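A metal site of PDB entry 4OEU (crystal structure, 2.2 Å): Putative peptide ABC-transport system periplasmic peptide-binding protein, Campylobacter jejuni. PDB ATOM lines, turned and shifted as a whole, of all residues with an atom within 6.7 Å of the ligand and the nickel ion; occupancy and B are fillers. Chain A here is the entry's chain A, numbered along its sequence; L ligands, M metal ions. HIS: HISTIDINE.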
ATOM      1  N   ASN A  13       3.977 -13.532  24.785  1.00  0.00           N
ATOM      2  CA  ASN A  13       3.646 -12.355  23.985  1.00  0.00           C
ATOM      3  C   ASN A  13       3.102 -12.718  22.610  1.00  0.00           C
ATOM      4  O   ASN A  13       3.615 -13.620  21.939  1.00  0.00           O
ATOM      5  CB  ASN A  13       4.867 -11.440  23.822  1.00  0.00           C
ATOM      6  CG  ASN A  13       5.110 -10.573  25.036  1.00  0.00           C
ATOM      7  OD1 ASN A  13       5.859 -10.942  25.937  1.00  0.00           O
ATOM      8  ND2 ASN A  13       4.443  -9.418  25.082  1.00  0.00           N
ATOM      9  N   GLU A  24       8.925  -6.382  16.851  1.00  0.00           N
ATOM     10  CA  GLU A  24       9.331  -5.597  17.996  1.00  0.00           C
ATOM     11  C   GLU A  24      10.072  -6.465  18.998  1.00  0.00           C
ATOM     12  O   GLU A  24      10.056  -6.190  20.191  1.00  0.00           O
ATOM     13  CB  GLU A  24       8.108  -4.959  18.639  1.00  0.00           C
ATOM     14  CG  GLU A  24       7.435  -3.925  17.778  1.00  0.00           C
ATOM     15  CD  GLU A  24       6.102  -3.484  18.340  1.00  0.00           C
ATOM     16  OE1 GLU A  24       5.521  -4.232  19.155  1.00  0.00           O
ATOM     17  OE2 GLU A  24       5.623  -2.389  17.969  1.00  0.00           O
ATOM     18  N   ASP A  25      10.687  -7.540  18.499  1.00  0.00           N
ATOM     19  CA  ASP A  25      11.416  -8.491  19.340  1.00  0.00           C
ATOM     20  C   ASP A  25      10.562  -9.005  20.508  1.00  0.00           C
ATOM     21  O   ASP A  25      11.089  -9.303  21.585  1.00  0.00           O
ATOM     22  CB  ASP A  25      12.698  -7.862  19.870  1.00  0.00           C
ATOM     23  CG  ASP A  25      13.712  -7.584  18.775  1.00  0.00           C
ATOM     24  OD1 ASP A  25      13.682  -8.289  17.745  1.00  0.00           O
ATOM     25  OD2 ASP A  25      14.540  -6.668  18.965  1.00  0.00           O
ATOM     26  N   HIS A  26       9.259  -9.105  20.303  1.00  0.00           N
ATOM     27  CA  HIS A  26       8.362  -9.571  21.346  1.00  0.00           C
ATOM     28  C   HIS A  26       7.525 -10.745  20.884  1.00  0.00           C
ATOM     29  O   HIS A  26       6.401 -10.916  21.334  1.00  0.00           O
ATOM     30  CB  HIS A  26       7.428  -8.445  21.811  1.00  0.00           C
ATOM     31  CG  HIS A  26       8.002  -7.566  22.879  1.00  0.00           C
ATOM     32  ND1 HIS A  26       8.958  -6.606  22.614  1.00  0.00           N
ATOM     33  CD2 HIS A  26       7.751  -7.496  24.202  1.00  0.00           C
ATOM     34  CE1 HIS A  26       9.270  -5.977  23.736  1.00  0.00           C
ATOM     35  NE2 HIS A  26       8.557  -6.508  24.723  1.00  0.00           N
ATOM     36  N   ASP A 240      18.306 -10.081  28.784  1.00  0.00           N
ATOM     37  CA  ASP A 240      17.118  -9.429  29.341  1.00  0.00           C
ATOM     38  C   ASP A 240      17.391  -8.870  30.724  1.00  0.00           C
ATOM     39  O   ASP A 240      17.882  -9.579  31.607  1.00  0.00           O
ATOM     40  CB  ASP A 240      15.952 -10.416  29.409  1.00  0.00           C
ATOM     41  CG  ASP A 240      14.616  -9.727  29.638  1.00  0.00           C
ATOM     42  OD1 ASP A 240      14.543  -8.480  29.546  1.00  0.00           O
ATOM     43  OD2 ASP A 240      13.634 -10.441  29.911  1.00  0.00           O
ATOM     44  N   ARG A 242      15.679  -6.339  34.026  1.00  0.00           N
ATOM     45  CA  ARG A 242      14.507  -5.664  34.572  1.00  0.00           C
ATOM     46  C   ARG A 242      14.980  -4.361  35.200  1.00  0.00           C
ATOM     47  O   ARG A 242      16.104  -4.263  35.684  1.00  0.00           O
ATOM     48  CB  ARG A 242      13.774  -6.535  35.617  1.00  0.00           C
ATOM     49  CG  ARG A 242      13.173  -7.801  35.041  1.00  0.00           C
ATOM     50  CD  ARG A 242      11.895  -7.503  34.253  1.00  0.00           C
ATOM     51  NE  ARG A 242      11.517  -8.638  33.404  1.00  0.00           N
ATOM     52  CZ  ARG A 242      12.067  -8.878  32.223  1.00  0.00           C
ATOM     53  NH1 ARG A 242      12.991  -8.062  31.749  1.00  0.00           N
ATOM     54  NH2 ARG A 242      11.674  -9.926  31.502  1.00  0.00           N
ATOM     55  N   MET A 338       3.084  -5.323  35.576  1.00  0.00           N
ATOM     56  CA  MET A 338       2.199  -6.253  34.896  1.00  0.00           C
ATOM     57  C   MET A 338       1.860  -7.389  35.863  1.00  0.00           C
ATOM     58  O   MET A 338       2.735  -8.167  36.270  1.00  0.00           O
ATOM     59  CB  MET A 338       2.837  -6.779  33.609  1.00  0.00           C
ATOM     60  CG  MET A 338       3.159  -5.656  32.617  1.00  0.00           C
ATOM     61  SD  MET A 338       3.994  -6.196  31.099  1.00  0.00           S
ATOM     62  CE  MET A 338       5.034  -7.502  31.745  1.00  0.00           C
ATOM     63  N   ARG A 344       7.803  -9.186  38.275  1.00  0.00           N
ATOM     64  CA  ARG A 344       7.632  -7.737  38.239  1.00  0.00           C
ATOM     65  C   ARG A 344       6.823  -7.208  39.421  1.00  0.00           C
ATOM     66  O   ARG A 344       7.171  -6.176  39.989  1.00  0.00           O
ATOM     67  CB  ARG A 344       7.005  -7.303  36.918  1.00  0.00           C
ATOM     68  CG  ARG A 344       7.745  -7.839  35.701  1.00  0.00           C
ATOM     69  CD  ARG A 344       7.643  -6.868  34.541  1.00  0.00           C
ATOM     70  NE  ARG A 344       8.105  -7.474  33.293  1.00  0.00           N
ATOM     71  CZ  ARG A 344       8.373  -6.792  32.186  1.00  0.00           C
ATOM     72  NH1 ARG A 344       8.782  -7.442  31.093  1.00  0.00           N
ATOM     73  NH2 ARG A 344       8.257  -5.479  32.169  1.00  0.00           N
ATOM     74  N   ALA A 369      -0.902  -7.044  31.603  1.00  0.00           N
ATOM     75  CA  ALA A 369      -0.249  -6.470  30.429  1.00  0.00           C
ATOM     76  C   ALA A 369      -1.281  -6.204  29.337  1.00  0.00           C
ATOM     77  O   ALA A 369      -2.163  -7.030  29.093  1.00  0.00           O
ATOM     78  CB  ALA A 369       0.849  -7.407  29.913  1.00  0.00           C
ATOM     79  N   GLY A 370      -1.195  -5.032  28.728  1.00  0.00           N
ATOM     80  CA  GLY A 370      -2.145  -4.638  27.695  1.00  0.00           C
ATOM     81  C   GLY A 370      -3.360  -3.875  28.197  1.00  0.00           C
ATOM     82  O   GLY A 370      -4.114  -3.333  27.399  1.00  0.00           O
ATOM     83  N   TYR A 374       1.670   2.156  29.619  1.00  0.00           N
ATOM     84  CA  TYR A 374       2.791   2.309  30.538  1.00  0.00           C
ATOM     85  C   TYR A 374       3.643   3.548  30.231  1.00  0.00           C
ATOM     86  O   TYR A 374       4.521   3.909  31.030  1.00  0.00           O
ATOM     87  CB  TYR A 374       3.673   1.055  30.545  1.00  0.00           C
ATOM     88  CG  TYR A 374       3.851   0.410  29.210  1.00  0.00           C
ATOM     89  CD1 TYR A 374       4.849   0.839  28.347  1.00  0.00           C
ATOM     90  CD2 TYR A 374       3.029  -0.631  28.799  1.00  0.00           C
ATOM     91  CE1 TYR A 374       5.021   0.247  27.110  1.00  0.00           C
ATOM     92  CE2 TYR A 374       3.195  -1.231  27.566  1.00  0.00           C
ATOM     93  CZ  TYR A 374       4.201  -0.783  26.727  1.00  0.00           C
ATOM     94  OH  TYR A 374       4.392  -1.361  25.493  1.00  0.00           O
ATOM     95  N   PHE A 380       7.337   2.525  35.917  1.00  0.00           N
ATOM     96  CA  PHE A 380       6.920   1.251  35.348  1.00  0.00           C
ATOM     97  C   PHE A 380       8.021   0.221  35.459  1.00  0.00           C
ATOM     98  O   PHE A 380       9.189   0.503  35.165  1.00  0.00           O
ATOM     99  CB  PHE A 380       6.511   1.457  33.875  1.00  0.00           C
ATOM    100  CG  PHE A 380       6.165   0.192  33.132  1.00  0.00           C
ATOM    101  CD1 PHE A 380       5.012  -0.524  33.422  1.00  0.00           C
ATOM    102  CD2 PHE A 380       6.965  -0.243  32.074  1.00  0.00           C
ATOM    103  CE1 PHE A 380       4.674  -1.674  32.707  1.00  0.00           C
ATOM    104  CE2 PHE A 380       6.632  -1.386  31.355  1.00  0.00           C
ATOM    105  CZ  PHE A 380       5.498  -2.101  31.676  1.00  0.00           C
ATOM    106  N   LEU A 381       7.675  -0.963  35.935  1.00  0.00           N
ATOM    107  CA  LEU A 381       8.669  -2.003  36.005  1.00  0.00           C
ATOM    108  C   LEU A 381       8.876  -2.618  34.610  1.00  0.00           C
ATOM    109  O   LEU A 381       8.132  -3.504  34.171  1.00  0.00           O
ATOM    110  CB  LEU A 381       8.288  -3.064  37.009  1.00  0.00           C
ATOM    111  CG  LEU A 381       9.596  -3.556  37.604  1.00  0.00           C
ATOM    112  CD1 LEU A 381      10.208  -2.516  38.546  1.00  0.00           C
ATOM    113  CD2 LEU A 381       9.336  -4.806  38.316  1.00  0.00           C
ATOM    114  N   ILE A 382       9.929  -2.142  33.952  1.00  0.00           N
ATOM    115  CA  ILE A 382      10.147  -2.363  32.543  1.00  0.00           C
ATOM    116  C   ILE A 382      11.207  -3.431  32.325  1.00  0.00           C
ATOM    117  O   ILE A 382      11.874  -3.860  33.280  1.00  0.00           O
ATOM    118  CB  ILE A 382      10.582  -1.054  31.854  1.00  0.00           C
ATOM    119  CG1 ILE A 382      10.280  -1.085  30.350  1.00  0.00           C
ATOM    120  CG2 ILE A 382      12.055  -0.785  32.113  1.00  0.00           C
ATOM    121  CD1 ILE A 382      10.235   0.291  29.722  1.00  0.00           C
ATOM    122  N   GLY A 383      11.324  -3.884  31.078  1.00  0.00           N
ATOM    123  CA  GLY A 383      12.373  -4.812  30.671  1.00  0.00           C
ATOM    124  C   GLY A 383      12.767  -4.610  29.221  1.00  0.00           C
ATOM    125  O   GLY A 383      11.942  -4.252  28.376  1.00  0.00           O
ATOM    126  N   TRP A 384      14.046  -4.854  28.930  1.00  0.00           N
ATOM    127  CA  TRP A 384      14.596  -4.835  27.575  1.00  0.00           C
ATOM    128  C   TRP A 384      15.831  -5.719  27.503  1.00  0.00           C
ATOM    129  O   TRP A 384      16.296  -6.222  28.530  1.00  0.00           O
ATOM    130  CB  TRP A 384      14.998  -3.412  27.157  1.00  0.00           C
ATOM    131  CG  TRP A 384      13.877  -2.424  27.012  1.00  0.00           C
ATOM    132  CD1 TRP A 384      13.621  -1.361  27.820  1.00  0.00           C
ATOM    133  CD2 TRP A 384      12.894  -2.388  25.979  1.00  0.00           C
ATOM    134  NE1 TRP A 384      12.526  -0.664  27.359  1.00  0.00           N
ATOM    135  CE2 TRP A 384      12.058  -1.276  26.234  1.00  0.00           C
ATOM    136  CE3 TRP A 384      12.626  -3.192  24.861  1.00  0.00           C
ATOM    137  CZ2 TRP A 384      10.967  -0.953  25.418  1.00  0.00           C
ATOM    138  CZ3 TRP A 384      11.542  -2.857  24.051  1.00  0.00           C
ATOM    139  CH2 TRP A 384      10.734  -1.749  24.337  1.00  0.00           C
ATOM    140  N   PHE A 413       9.587   5.036  26.310  1.00  0.00           N
ATOM    141  CA  PHE A 413       8.282   5.146  26.965  1.00  0.00           C
ATOM    142  C   PHE A 413       8.305   6.129  28.151  1.00  0.00           C
ATOM    143  O   PHE A 413       7.264   6.635  28.570  1.00  0.00           O
ATOM    144  CB  PHE A 413       7.782   3.763  27.408  1.00  0.00           C
ATOM    145  CG  PHE A 413       7.507   2.809  26.267  1.00  0.00           C
ATOM    146  CD1 PHE A 413       6.760   3.222  25.162  1.00  0.00           C
ATOM    147  CD2 PHE A 413       8.009   1.519  26.271  1.00  0.00           C
ATOM    148  CE1 PHE A 413       6.499   2.348  24.095  1.00  0.00           C
ATOM    149  CE2 PHE A 413       7.763   0.650  25.211  1.00  0.00           C
ATOM    150  CZ  PHE A 413       7.003   1.065  24.118  1.00  0.00           C
ATOM    151  N   HIS A 480      15.101 -10.343  25.180  1.00  0.00           N
ATOM    152  CA  HIS A 480      14.034  -9.856  26.035  1.00  0.00           C
ATOM    153  C   HIS A 480      12.807 -10.792  26.010  1.00  0.00           C
ATOM    154  O   HIS A 480      12.389 -11.251  24.947  1.00  0.00           O
ATOM    155  CB  HIS A 480      13.668  -8.429  25.590  1.00  0.00           C
ATOM    156  CG  HIS A 480      12.547  -7.810  26.340  1.00  0.00           C
ATOM    157  ND1 HIS A 480      12.470  -7.809  27.718  1.00  0.00           N
ATOM    158  CD2 HIS A 480      11.452  -7.122  25.915  1.00  0.00           C
ATOM    159  CE1 HIS A 480      11.381  -7.180  28.102  1.00  0.00           C
ATOM    160  NE2 HIS A 480      10.751  -6.742  27.030  1.00  0.00           N
ATOM    161  N   HIS A 481      12.269 -11.086  27.197  1.00  0.00           N
ATOM    162  CA  HIS A 481      11.165 -12.050  27.402  1.00  0.00           C
ATOM    163  C   HIS A 481      11.561 -13.489  27.054  1.00  0.00           C
ATOM    164  O   HIS A 481      10.711 -14.368  26.992  1.00  0.00           O
ATOM    165  CB  HIS A 481       9.921 -11.690  26.574  1.00  0.00           C
ATOM    166  CG  HIS A 481       9.246 -10.429  26.990  1.00  0.00           C
ATOM    167  ND1 HIS A 481       8.533 -10.299  28.168  1.00  0.00           N
ATOM    168  CD2 HIS A 481       9.165  -9.222  26.371  1.00  0.00           C
ATOM    169  CE1 HIS A 481       8.034  -9.077  28.246  1.00  0.00           C
ATOM    170  NE2 HIS A 481       8.411  -8.402  27.176  1.00  0.00           N
HETATM  171  N   HIS L   1       9.404  -4.462  26.527  1.00  0.00           N
HETATM  172  CA  HIS L   1       8.862  -3.662  27.625  1.00  0.00           C
HETATM  173  C   HIS L   1       8.810  -4.466  28.904  1.00  0.00           C
HETATM  174  O   HIS L   1       8.950  -5.683  28.857  1.00  0.00           O
HETATM  175  CB  HIS L   1       7.450  -3.176  27.272  1.00  0.00           C
HETATM  176  CG  HIS L   1       6.443  -4.276  27.176  1.00  0.00           C
HETATM  177  ND1 HIS L   1       6.757  -5.551  26.723  1.00  0.00           N
HETATM  178  CD2 HIS L   1       5.116  -4.319  27.461  1.00  0.00           C
HETATM  179  CE1 HIS L   1       5.688  -6.302  26.737  1.00  0.00           C
HETATM  180  NE2 HIS L   1       4.675  -5.590  27.187  1.00  0.00           N
HETATM  181  OXT HIS L   1       8.592  -3.948  30.003  1.00  0.00           O
HETATM  182 NI    NI M   1       8.748  -6.273  26.729  1.00  0.00          NI
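N of Gly 383 sits at hydrogen-bond distance from OXT of the ligand (2.9 Å). The backbone carbonyl oxygen of Gly 383 sits close to a nitrogen (N) of the ligand, 3.1 Å away. The guanidinium group of Arg 344 is in salt-bridge range of an oxygen (OXT) of the ligand, 2.7 Å away.
The guanidinium group of Arg 344 is in hydrogen-bond range of the backbone carbonyl oxygen of Leu 381 (2.8 Å). OD2 of Asp 240 sits at hydrogen-bond distance from N of His 481 (3.1 Å). A ring nitrogen (NE2) of His 480 lies close to the backbone carbonyl oxygen (O) of Gly 383, at 3.1 Å. ND1 of His 26 sits at hydrogen-bond distance from O of Glu 24 (2.7 Å). The side-chain carboxylate (OD1) of Asp 240 lies within hydrogen-bond range of a ring nitrogen (ND1) of His 480, 2.8 Å away.
Asn 13 touches the ligand. Tyr 374 touches the ligand (OH to CD2, 3.6 Å). CE2 of Phe 380 touches OXT of the ligand, 3.5 Å away. CG1 of Ile 382 touches OXT of the ligand, at 3.3 Å. CZ3 of Trp 384 touches N of the ligand, 3.6 Å away. Ten residues have an atom within 4 Å of the ligand: Asn 13, His 26, Arg 344, Tyr 374, Phe 380, Ile 382, Gly 383, Trp 384, His 480 and His 481. The nearest printed residue that does not touch the ligand is Met 338 (4.02 Å).
Of the 19 residues printed, 3 come within 4 Å of the nickel ion.
The nickel ion is bound by a nitrogen (N) of the ligand, a ring nitrogen (NE2) of His 26, a ring nitrogen (NE2) of His 480, a nitrogen (ND1) of the ligand, a ring nitrogen (NE2) of His 481 and an oxygen (O) of the ligand. The nickel ion has six donor atoms within binding distance.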
